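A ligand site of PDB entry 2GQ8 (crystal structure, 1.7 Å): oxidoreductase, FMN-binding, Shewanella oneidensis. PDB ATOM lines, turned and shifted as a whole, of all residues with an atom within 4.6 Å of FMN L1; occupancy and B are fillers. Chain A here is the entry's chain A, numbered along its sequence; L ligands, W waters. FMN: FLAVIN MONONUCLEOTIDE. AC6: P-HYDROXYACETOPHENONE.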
ATOM      1  N   PRO A  23      23.501   7.801  16.261  1.00  0.00           N
ATOM      2  CA  PRO A  23      22.208   8.001  16.928  1.00  0.00           C
ATOM      3  C   PRO A  23      21.502   6.673  17.180  1.00  0.00           C
ATOM      4  O   PRO A  23      21.823   5.675  16.557  1.00  0.00           O
ATOM      5  CB  PRO A  23      21.456   8.895  15.957  1.00  0.00           C
ATOM      6  CG  PRO A  23      21.911   8.352  14.626  1.00  0.00           C
ATOM      7  CD  PRO A  23      23.397   8.122  14.823  1.00  0.00           C
ATOM      8  N   PRO A  24      20.536   6.669  18.099  1.00  0.00           N
ATOM      9  CA  PRO A  24      19.771   5.470  18.438  1.00  0.00           C
ATOM     10  C   PRO A  24      19.043   4.922  17.216  1.00  0.00           C
ATOM     11  O   PRO A  24      18.346   5.674  16.538  1.00  0.00           O
ATOM     12  CB  PRO A  24      18.810   5.966  19.526  1.00  0.00           C
ATOM     13  CG  PRO A  24      18.617   7.401  19.180  1.00  0.00           C
ATOM     14  CD  PRO A  24      20.009   7.848  18.809  1.00  0.00           C
ATOM     15  N   MET A  25      19.220   3.635  16.933  1.00  0.00           N
ATOM     16  CA  MET A  25      18.551   3.029  15.793  1.00  0.00           C
ATOM     17  C   MET A  25      18.078   1.613  16.060  1.00  0.00           C
ATOM     18  O   MET A  25      18.870   0.682  16.171  1.00  0.00           O
ATOM     19  CB  MET A  25      19.444   3.050  14.547  1.00  0.00           C
ATOM     20  CG  MET A  25      19.649   4.455  14.009  1.00  0.00           C
ATOM     21  SD  MET A  25      20.672   4.498  12.520  1.00  0.00           S
ATOM     22  CE  MET A  25      22.289   4.012  13.205  1.00  0.00           C
ATOM     23  N   THR A  26      16.764   1.479  16.197  1.00  0.00           N
ATOM     24  CA  THR A  26      16.123   0.198  16.419  1.00  0.00           C
ATOM     25  C   THR A  26      16.455  -0.748  15.269  1.00  0.00           C
ATOM     26  O   THR A  26      16.260  -0.393  14.117  1.00  0.00           O
ATOM     27  CB  THR A  26      14.596   0.379  16.457  1.00  0.00           C
ATOM     28  OG1 THR A  26      14.238   1.129  17.610  1.00  0.00           O
ATOM     29  CG2 THR A  26      13.884  -0.983  16.499  1.00  0.00           C
ATOM     30  N   ARG A  27      16.953  -1.942  15.581  1.00  0.00           N
ATOM     31  CA  ARG A  27      17.277  -2.930  14.550  1.00  0.00           C
ATOM     32  C   ARG A  27      16.492  -4.220  14.779  1.00  0.00           C
ATOM     33  O   ARG A  27      16.524  -5.135  13.959  1.00  0.00           O
ATOM     34  CB  ARG A  27      18.785  -3.219  14.533  1.00  0.00           C
ATOM     35  CG  ARG A  27      19.660  -1.983  14.334  1.00  0.00           C
ATOM     36  CD  ARG A  27      19.276  -1.191  13.081  1.00  0.00           C
ATOM     37  NE  ARG A  27      19.312  -2.018  11.880  1.00  0.00           N
ATOM     38  CZ  ARG A  27      20.412  -2.298  11.181  1.00  0.00           C
ATOM     39  NH1 ARG A  27      21.581  -1.796  11.556  1.00  0.00           N
ATOM     40  NH2 ARG A  27      20.339  -3.109  10.140  1.00  0.00           N
ATOM     41  N   GLU A  57      20.047   1.721  20.422  1.00  0.00           N
ATOM     42  CA  GLU A  57      18.693   1.703  19.892  1.00  0.00           C
ATOM     43  C   GLU A  57      17.777   1.808  21.110  1.00  0.00           C
ATOM     44  O   GLU A  57      18.176   1.455  22.224  1.00  0.00           O
ATOM     45  CB  GLU A  57      18.448   0.368  19.212  1.00  0.00           C
ATOM     46  CG  GLU A  57      18.702  -0.809  20.153  1.00  0.00           C
ATOM     47  CD  GLU A  57      19.143  -2.055  19.425  1.00  0.00           C
ATOM     48  OE1 GLU A  57      18.265  -2.844  19.008  1.00  0.00           O
ATOM     49  OE2 GLU A  57      20.359  -2.236  19.251  1.00  0.00           O
ATOM     50  N   GLY A  58      16.553   2.259  20.903  1.00  0.00           N
ATOM     51  CA  GLY A  58      15.626   2.350  22.016  1.00  0.00           C
ATOM     52  C   GLY A  58      15.532   1.019  22.741  1.00  0.00           C
ATOM     53  O   GLY A  58      15.471  -0.038  22.113  1.00  0.00           O
ATOM     54  N   GLN A 100      19.412   4.269  25.295  1.00  0.00           N
ATOM     55  CA  GLN A 100      18.233   5.112  25.104  1.00  0.00           C
ATOM     56  C   GLN A 100      17.041   4.452  25.776  1.00  0.00           C
ATOM     57  O   GLN A 100      16.493   3.456  25.269  1.00  0.00           O
ATOM     58  CB  GLN A 100      17.904   5.353  23.622  1.00  0.00           C
ATOM     59  CG  GLN A 100      16.716   6.323  23.481  1.00  0.00           C
ATOM     60  CD  GLN A 100      16.219   6.502  22.070  1.00  0.00           C
ATOM     61  OE1 GLN A 100      15.766   5.550  21.426  1.00  0.00           O
ATOM     62  NE2 GLN A 100      16.282   7.745  21.586  1.00  0.00           N
ATOM     63  N   TRP A 102      13.458   3.779  26.617  1.00  0.00           N
ATOM     64  CA  TRP A 102      12.264   3.924  25.797  1.00  0.00           C
ATOM     65  C   TRP A 102      10.914   3.510  26.354  1.00  0.00           C
ATOM     66  O   TRP A 102      10.777   2.458  26.976  1.00  0.00           O
ATOM     67  CB  TRP A 102      12.530   3.103  24.528  1.00  0.00           C
ATOM     68  CG  TRP A 102      11.757   3.420  23.299  1.00  0.00           C
ATOM     69  CD1 TRP A 102      11.042   4.555  23.018  1.00  0.00           C
ATOM     70  CD2 TRP A 102      11.746   2.632  22.102  1.00  0.00           C
ATOM     71  NE1 TRP A 102      10.599   4.519  21.716  1.00  0.00           N
ATOM     72  CE2 TRP A 102      11.006   3.351  21.130  1.00  0.00           C
ATOM     73  CE3 TRP A 102      12.284   1.379  21.749  1.00  0.00           C
ATOM     74  CZ2 TRP A 102      10.807   2.864  19.828  1.00  0.00           C
ATOM     75  CZ3 TRP A 102      12.093   0.896  20.468  1.00  0.00           C
ATOM     76  CH2 TRP A 102      11.355   1.639  19.514  1.00  0.00           C
ATOM     77  N   HIS A 181      14.360   8.954  25.703  1.00  0.00           N
ATOM     78  CA  HIS A 181      13.679   9.168  24.432  1.00  0.00           C
ATOM     79  C   HIS A 181      12.393   9.947  24.724  1.00  0.00           C
ATOM     80  O   HIS A 181      11.411   9.380  25.204  1.00  0.00           O
ATOM     81  CB  HIS A 181      13.309   7.841  23.778  1.00  0.00           C
ATOM     82  CG  HIS A 181      12.971   7.967  22.324  1.00  0.00           C
ATOM     83  ND1 HIS A 181      12.667   9.176  21.731  1.00  0.00           N
ATOM     84  CD2 HIS A 181      12.935   7.036  21.338  1.00  0.00           C
ATOM     85  CE1 HIS A 181      12.444   8.986  20.438  1.00  0.00           C
ATOM     86  NE2 HIS A 181      12.602   7.697  20.177  1.00  0.00           N
ATOM     87  N   ASN A 184      10.199  11.711  18.789  1.00  0.00           N
ATOM     88  CA  ASN A 184       9.524  10.947  17.754  1.00  0.00           C
ATOM     89  C   ASN A 184       8.152  10.351  18.041  1.00  0.00           C
ATOM     90  O   ASN A 184       7.844   9.236  17.630  1.00  0.00           O
ATOM     91  CB  ASN A 184      10.478   9.871  17.241  1.00  0.00           C
ATOM     92  CG  ASN A 184      11.770  10.482  16.727  1.00  0.00           C
ATOM     93  OD1 ASN A 184      11.808  11.670  16.386  1.00  0.00           O
ATOM     94  ND2 ASN A 184      12.825   9.691  16.660  1.00  0.00           N
ATOM     95  N   ARG A 233      16.434  13.272  24.376  1.00  0.00           N
ATOM     96  CA  ARG A 233      16.177  13.487  22.950  1.00  0.00           C
ATOM     97  C   ARG A 233      14.791  14.090  22.733  1.00  0.00           C
ATOM     98  O   ARG A 233      13.812  13.618  23.323  1.00  0.00           O
ATOM     99  CB  ARG A 233      16.283  12.178  22.152  1.00  0.00           C
ATOM    100  CG  ARG A 233      16.390  12.437  20.649  1.00  0.00           C
ATOM    101  CD  ARG A 233      16.697  11.194  19.820  1.00  0.00           C
ATOM    102  NE  ARG A 233      17.537  11.534  18.667  1.00  0.00           N
ATOM    103  CZ  ARG A 233      17.556  10.883  17.503  1.00  0.00           C
ATOM    104  NH1 ARG A 233      16.772   9.840  17.290  1.00  0.00           N
ATOM    105  NH2 ARG A 233      18.387  11.284  16.550  1.00  0.00           N
ATOM    106  N   ALA A 270      16.197  15.437  17.289  1.00  0.00           N
ATOM    107  CA  ALA A 270      15.936  14.581  16.132  1.00  0.00           C
ATOM    108  C   ALA A 270      15.288  15.512  15.124  1.00  0.00           C
ATOM    109  O   ALA A 270      14.095  15.825  15.204  1.00  0.00           O
ATOM    110  CB  ALA A 270      14.987  13.449  16.521  1.00  0.00           C
ATOM    111  N   VAL A 272      15.139  15.108  11.701  1.00  0.00           N
ATOM    112  CA  VAL A 272      14.469  14.413  10.615  1.00  0.00           C
ATOM    113  C   VAL A 272      14.085  13.039  11.136  1.00  0.00           C
ATOM    114  O   VAL A 272      14.804  12.452  11.936  1.00  0.00           O
ATOM    115  CB  VAL A 272      15.437  14.229   9.404  1.00  0.00           C
ATOM    116  CG1 VAL A 272      14.770  13.369   8.323  1.00  0.00           C
ATOM    117  CG2 VAL A 272      15.832  15.580   8.835  1.00  0.00           C
ATOM    118  N   ASP A 273      12.928  12.556  10.709  1.00  0.00           N
ATOM    119  CA  ASP A 273      12.510  11.209  11.086  1.00  0.00           C
ATOM    120  C   ASP A 273      12.108  10.596   9.750  1.00  0.00           C
ATOM    121  O   ASP A 273      11.089  10.975   9.180  1.00  0.00           O
ATOM    122  CB  ASP A 273      11.328  11.221  12.048  1.00  0.00           C
ATOM    123  CG  ASP A 273      11.205   9.928  12.819  1.00  0.00           C
ATOM    124  OD1 ASP A 273      10.079   9.596  13.249  1.00  0.00           O
ATOM    125  OD2 ASP A 273      12.233   9.229  13.006  1.00  0.00           O
ATOM    126  N   TRP A 274      12.932   9.673   9.253  1.00  0.00           N
ATOM    127  CA  TRP A 274      12.703   9.031   7.956  1.00  0.00           C
ATOM    128  C   TRP A 274      12.669  10.087   6.857  1.00  0.00           C
ATOM    129  O   TRP A 274      13.709  10.679   6.549  1.00  0.00           O
ATOM    130  CB  TRP A 274      11.404   8.209   7.982  1.00  0.00           C
ATOM    131  CG  TRP A 274      11.506   7.051   8.926  1.00  0.00           C
ATOM    132  CD1 TRP A 274      10.907   6.923  10.144  1.00  0.00           C
ATOM    133  CD2 TRP A 274      12.288   5.866   8.740  1.00  0.00           C
ATOM    134  NE1 TRP A 274      11.271   5.730  10.725  1.00  0.00           N
ATOM    135  CE2 TRP A 274      12.117   5.058   9.884  1.00  0.00           C
ATOM    136  CE3 TRP A 274      13.120   5.400   7.704  1.00  0.00           C
ATOM    137  CZ2 TRP A 274      12.750   3.814  10.039  1.00  0.00           C
ATOM    138  CZ3 TRP A 274      13.743   4.162   7.852  1.00  0.00           C
ATOM    139  CH2 TRP A 274      13.555   3.394   9.012  1.00  0.00           C
ATOM    140  N   ALA A 299      20.649  15.372  14.714  1.00  0.00           N
ATOM    141  CA  ALA A 299      20.727  14.260  13.773  1.00  0.00           C
ATOM    142  C   ALA A 299      19.574  14.399  12.788  1.00  0.00           C
ATOM    143  O   ALA A 299      18.482  14.825  13.170  1.00  0.00           O
ATOM    144  CB  ALA A 299      20.639  12.911  14.514  1.00  0.00           C
ATOM    145  N   GLY A 300      19.830  14.057  11.527  1.00  0.00           N
ATOM    146  CA  GLY A 300      18.791  14.153  10.514  1.00  0.00           C
ATOM    147  C   GLY A 300      19.311  14.664   9.176  1.00  0.00           C
ATOM    148  O   GLY A 300      19.463  15.879   8.976  1.00  0.00           O
ATOM    149  N   ARG A 301      19.568  13.732   8.270  1.00  0.00           N
ATOM    150  CA  ARG A 301      20.061  14.026   6.931  1.00  0.00           C
ATOM    151  C   ARG A 301      21.323  14.864   6.863  1.00  0.00           C
ATOM    152  O   ARG A 301      21.501  15.654   5.935  1.00  0.00           O
ATOM    153  CB  ARG A 301      18.975  14.702   6.093  1.00  0.00           C
ATOM    154  CG  ARG A 301      17.774  13.813   5.809  1.00  0.00           C
ATOM    155  CD  ARG A 301      18.175  12.542   5.058  1.00  0.00           C
ATOM    156  NE  ARG A 301      17.011  11.864   4.490  1.00  0.00           N
ATOM    157  CZ  ARG A 301      17.007  10.603   4.055  1.00  0.00           C
ATOM    158  NH1 ARG A 301      18.108   9.870   4.115  1.00  0.00           N
ATOM    159  NH2 ARG A 301      15.896  10.093   3.544  1.00  0.00           N
ATOM    160  N   GLY A 320      24.835  13.581  14.743  1.00  0.00           N
ATOM    161  CA  GLY A 320      24.587  12.163  14.579  1.00  0.00           C
ATOM    162  C   GLY A 320      24.292  11.840  13.112  1.00  0.00           C
ATOM    163  O   GLY A 320      23.704  12.641  12.402  1.00  0.00           O
ATOM    164  N   PHE A 321      24.749  10.670  12.675  1.00  0.00           N
ATOM    165  CA  PHE A 321      24.538  10.182  11.309  1.00  0.00           C
ATOM    166  C   PHE A 321      23.922   8.814  11.526  1.00  0.00           C
ATOM    167  O   PHE A 321      24.570   7.905  12.047  1.00  0.00           O
ATOM    168  CB  PHE A 321      25.872  10.030  10.577  1.00  0.00           C
ATOM    169  CG  PHE A 321      26.628  11.310  10.429  1.00  0.00           C
ATOM    170  CD1 PHE A 321      26.454  12.091   9.289  1.00  0.00           C
ATOM    171  CD2 PHE A 321      27.497  11.739  11.424  1.00  0.00           C
ATOM    172  CE1 PHE A 321      27.152  13.292   9.146  1.00  0.00           C
ATOM    173  CE2 PHE A 321      28.202  12.942  11.286  1.00  0.00           C
ATOM    174  CZ  PHE A 321      28.024  13.711  10.141  1.00  0.00           C
ATOM    175  N   GLY A 322      22.655   8.680  11.134  1.00  0.00           N
ATOM    176  CA  GLY A 322      21.956   7.423  11.348  1.00  0.00           C
ATOM    177  C   GLY A 322      22.095   6.415  10.236  1.00  0.00           C
ATOM    178  O   GLY A 322      22.903   5.494  10.309  1.00  0.00           O
ATOM    179  N   ARG A 323      21.289   6.585   9.196  1.00  0.00           N
ATOM    180  CA  ARG A 323      21.335   5.644   8.079  1.00  0.00           C
ATOM    181  C   ARG A 323      22.746   5.428   7.537  1.00  0.00           C
ATOM    182  O   ARG A 323      23.112   4.298   7.227  1.00  0.00           O
ATOM    183  CB  ARG A 323      20.327   6.089   7.023  1.00  0.00           C
ATOM    184  CG  ARG A 323      18.916   5.765   7.515  1.00  0.00           C
ATOM    185  CD  ARG A 323      17.799   6.509   6.806  1.00  0.00           C
ATOM    186  NE  ARG A 323      17.682   7.893   7.260  1.00  0.00           N
ATOM    187  CZ  ARG A 323      16.685   8.699   6.916  1.00  0.00           C
ATOM    188  NH1 ARG A 323      16.657   9.953   7.375  1.00  0.00           N
ATOM    189  NH2 ARG A 323      15.716   8.263   6.127  1.00  0.00           N
ATOM    190  N   PRO A 324      23.557   6.500   7.446  1.00  0.00           N
ATOM    191  CA  PRO A 324      24.907   6.250   6.939  1.00  0.00           C
ATOM    192  C   PRO A 324      25.722   5.326   7.854  1.00  0.00           C
ATOM    193  O   PRO A 324      26.572   4.580   7.378  1.00  0.00           O
ATOM    194  CB  PRO A 324      25.514   7.663   6.867  1.00  0.00           C
ATOM    195  CG  PRO A 324      24.310   8.503   6.521  1.00  0.00           C
ATOM    196  CD  PRO A 324      23.265   7.947   7.481  1.00  0.00           C
ATOM    197  N   ILE A 326      24.527   2.845   9.511  1.00  0.00           N
ATOM    198  CA  ILE A 326      24.068   1.472   9.358  1.00  0.00           C
ATOM    199  C   ILE A 326      24.910   0.777   8.298  1.00  0.00           C
ATOM    200  O   ILE A 326      25.400  -0.336   8.508  1.00  0.00           O
ATOM    201  CB  ILE A 326      22.573   1.437   8.942  1.00  0.00           C
ATOM    202  CG1 ILE A 326      21.712   1.939  10.104  1.00  0.00           C
ATOM    203  CG2 ILE A 326      22.158   0.017   8.515  1.00  0.00           C
ATOM    204  CD1 ILE A 326      20.225   1.941   9.834  1.00  0.00           C
ATOM    205  N   LEU A 349      16.729  -3.629   7.743  1.00  0.00           N
ATOM    206  CA  LEU A 349      16.829  -2.726   8.887  1.00  0.00           C
ATOM    207  C   LEU A 349      16.293  -3.385  10.150  1.00  0.00           C
ATOM    208  O   LEU A 349      16.873  -3.241  11.226  1.00  0.00           O
ATOM    209  CB  LEU A 349      16.038  -1.442   8.641  1.00  0.00           C
ATOM    210  CG  LEU A 349      16.634  -0.456   7.636  1.00  0.00           C
ATOM    211  CD1 LEU A 349      15.650   0.679   7.403  1.00  0.00           C
ATOM    212  CD2 LEU A 349      17.969   0.100   8.161  1.00  0.00           C
ATOM    213  N   PHE A 350      15.182  -4.107  10.020  1.00  0.00           N
ATOM    214  CA  PHE A 350      14.543  -4.745  11.171  1.00  0.00           C
ATOM    215  C   PHE A 350      14.430  -6.248  11.111  1.00  0.00           C
ATOM    216  O   PHE A 350      14.071  -6.828  10.069  1.00  0.00           O
ATOM    217  CB  PHE A 350      13.134  -4.177  11.379  1.00  0.00           C
ATOM    218  CG  PHE A 350      13.077  -2.688  11.369  1.00  0.00           C
ATOM    219  CD1 PHE A 350      12.474  -2.011  10.311  1.00  0.00           C
ATOM    220  CD2 PHE A 350      13.613  -1.953  12.414  1.00  0.00           C
ATOM    221  CE1 PHE A 350      12.413  -0.620  10.285  1.00  0.00           C
ATOM    222  CE2 PHE A 350      13.560  -0.556  12.408  1.00  0.00           C
ATOM    223  CZ  PHE A 350      12.960   0.109  11.336  1.00  0.00           C
HETATM  224  N1  FMN L   1      15.500   7.362  16.812  1.00  0.00           N
HETATM  225  C2  FMN L   1      15.429   7.185  18.211  1.00  0.00           C
HETATM  226  O2  FMN L   1      15.399   8.104  18.966  1.00  0.00           O
HETATM  227  N3  FMN L   1      15.286   5.856  18.695  1.00  0.00           N
HETATM  228  C4  FMN L   1      15.570   4.753  17.972  1.00  0.00           C
HETATM  229  O4  FMN L   1      15.255   3.473  18.408  1.00  0.00           O
HETATM  230  C4A FMN L   1      15.472   4.867  16.445  1.00  0.00           C
HETATM  231  N5  FMN L   1      15.306   3.808  15.593  1.00  0.00           N
HETATM  232  C5A FMN L   1      15.601   4.027  14.286  1.00  0.00           C
HETATM  233  C6  FMN L   1      15.624   2.761  13.423  1.00  0.00           C
HETATM  234  C7  FMN L   1      16.011   2.947  12.044  1.00  0.00           C
HETATM  235  C7M FMN L   1      16.349   1.686  11.266  1.00  0.00           C
HETATM  236  C8  FMN L   1      16.490   4.190  11.506  1.00  0.00           C
HETATM  237  C8M FMN L   1      16.945   4.621  10.088  1.00  0.00           C
HETATM  238  C9  FMN L   1      16.325   5.383  12.263  1.00  0.00           C
HETATM  239  C9A FMN L   1      15.830   5.361  13.705  1.00  0.00           C
HETATM  240  N10 FMN L   1      15.818   6.452  14.660  1.00  0.00           N
HETATM  241  C10 FMN L   1      15.634   6.302  16.019  1.00  0.00           C
HETATM  242  C1' FMN L   1      16.038   7.825  14.182  1.00  0.00           C
HETATM  243  C2' FMN L   1      17.547   8.061  14.081  1.00  0.00           C
HETATM  244  O2' FMN L   1      18.187   8.097  15.353  1.00  0.00           O
HETATM  245  C3' FMN L   1      17.852   9.366  13.322  1.00  0.00           C
HETATM  246  O3' FMN L   1      17.379  10.504  14.099  1.00  0.00           O
HETATM  247  C4' FMN L   1      17.305   9.457  11.910  1.00  0.00           C
HETATM  248  O4' FMN L   1      17.611   8.244  11.177  1.00  0.00           O
HETATM  249  C5' FMN L   1      17.714  10.674  11.121  1.00  0.00           C
HETATM  250  O5' FMN L   1      19.132  10.669  10.867  1.00  0.00           O
HETATM  251  P   FMN L   1      19.728  10.181   9.467  1.00  0.00           P
HETATM  252  O1P FMN L   1      19.487   8.716   9.329  1.00  0.00           O
HETATM  253  O2P FMN L   1      19.090  11.000   8.371  1.00  0.00           O
HETATM  254  O3P FMN L   1      21.236  10.535   9.594  1.00  0.00           O
HETATM  255  C1  AC6 L   2      12.238   6.091  16.862  1.00  0.00           C
HETATM  256  C2  AC6 L   2      12.246   6.403  15.335  1.00  0.00           C
HETATM  257  C3  AC6 L   2      12.123   5.241  14.573  1.00  0.00           C
HETATM  258  C4  AC6 L   2      11.922   3.938  15.063  1.00  0.00           C
HETATM  259  C5  AC6 L   2      11.968   3.763  16.457  1.00  0.00           C
HETATM  260  C6  AC6 L   2      12.132   4.797  17.383  1.00  0.00           C
HETATM  261  O1  AC6 L   2      12.473   7.225  17.544  1.00  0.00           O
HETATM  262  O2  AC6 L   2      11.561   2.995  12.960  1.00  0.00           O
HETATM  263  C7  AC6 L   2      11.598   2.744  14.349  1.00  0.00           C
HETATM  264  C8  AC6 L   2      11.236   1.279  14.637  1.00  0.00           C
HETATM  265  O   HOH W   1      22.681  11.259   7.357  1.00  0.00           O
HETATM  266  O   HOH W   2      13.511   7.093  11.970  1.00  0.00           O
HETATM  267  O   HOH W   3      20.191  10.214   5.836  1.00  0.00           O
HETATM  268  O   HOH W   4      22.119  13.004  10.255  1.00  0.00           O
HETATM  269  O   HOH W   5      14.901   7.923   9.994  1.00  0.00           O
HETATM  270  O   HOH W   6      14.545  10.697  14.051  1.00  0.00           O
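The backbone NH (N) of Thr 26 is in hydrogen-bond range of a nitrogen (N5) of FMN L1, 2.8 Å away.
A ring nitrogen (NE2) of His 181 sits at hydrogen-bond distance from an oxygen (O2) of FMN L1, at 3.1 Å.
O2' of FMN L1 sits at hydrogen-bond distance from O of Pro 24 (2.7 Å).
NE2 of His 181 is in hydrogen-bond range of O1 of AC6 L2 (2.7 Å).
N of Arg 301 lies within hydrogen-bond range of O2P of FMN L1, at 2.8 Å.
An oxygen (O1P) of FMN L1 sits at hydrogen-bond distance from the backbone NH (N) of Arg 323 (2.8 Å).
The side-chain amide nitrogen of Gln 100 lies within hydrogen-bond range of an oxygen (O2) of FMN L1 (2.8 Å).
O4 of FMN L1 sits at hydrogen-bond distance from OG1 of Thr 26 (2.7 Å).
The backbone NH (N) of Gly 58 sits at hydrogen-bond distance from an oxygen (O4) of FMN L1 (3.1 Å).
An oxygen (O3P) of FMN L1 lies within hydrogen-bond range of the backbone NH of Gly 322.
The guanidinium group of Arg 323 lies within salt-bridge range of an oxygen (O2P) of FMN L1 (2.8 Å).
The guanidinium group (NH2) of Arg 233 lies within hydrogen-bond range of an oxygen (O3') of FMN L1 (2.8 Å).
ND2 of Asn 184 sits at hydrogen-bond distance from O1 of AC6 L2 (2.6 Å).
N1 of FMN L1 lies close to O1 of AC6 L2, 3.1 Å away.
The backbone carbonyl oxygen (O) of Trp 274 sits at hydrogen-bond distance from the guanidinium group (NH1) of Arg 323, 3.1 Å away.
The guanidinium group (NE) of Arg 27 lies within hydrogen-bond range of the backbone carbonyl oxygen (O) of Leu 349.
The backbone NH (N) of Gly 58 lies close to the side-chain amide oxygen (OE1) of Gln 100, 3.4 Å away.
Residues that only touch FMN L1: Met 25, Pro 23, Val 272, Gly 300, Asn 184, Phe 321, Phe 350, Trp 274, Leu 349 and Pro 324.
Hydrophobic or aromatic side chains within 4 Å of FMN L1: Pro 23, Pro 24, Met 25, His 181, Trp 274, Pro 324, Leu 349 and Phe 350.
Along chain A the residues within 4 Å of FMN L1 span positions 23 to 350.
The nearest printed residue that does not touch FMN L1 is Glu 57 (4.1 Å).
Water W4 lies within hydrogen-bond range of the backbone carbonyl oxygen (O) of Gly 320, an oxygen (O3P) of FMN L1, the backbone NH (N) of Gly 300 and the backbone NH (N) of Arg 301.
Water W6 lies within hydrogen-bond range of O of Val 272 (2.8 Å), O3' of FMN L1 (2.8 Å), OD2 of Asp 273 (2.9 Å) and ND2 of Asn 184 (3.3 Å).
Water W3 bridges NH1 of Arg 301 and O2P of FMN L1.
Water W5 bridges N of Trp 274 and O4' of FMN L1.
Water W2 bridges OD2 of Asp 273 (2.7 Å) and NE1 of Trp 274 (2.9 Å).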
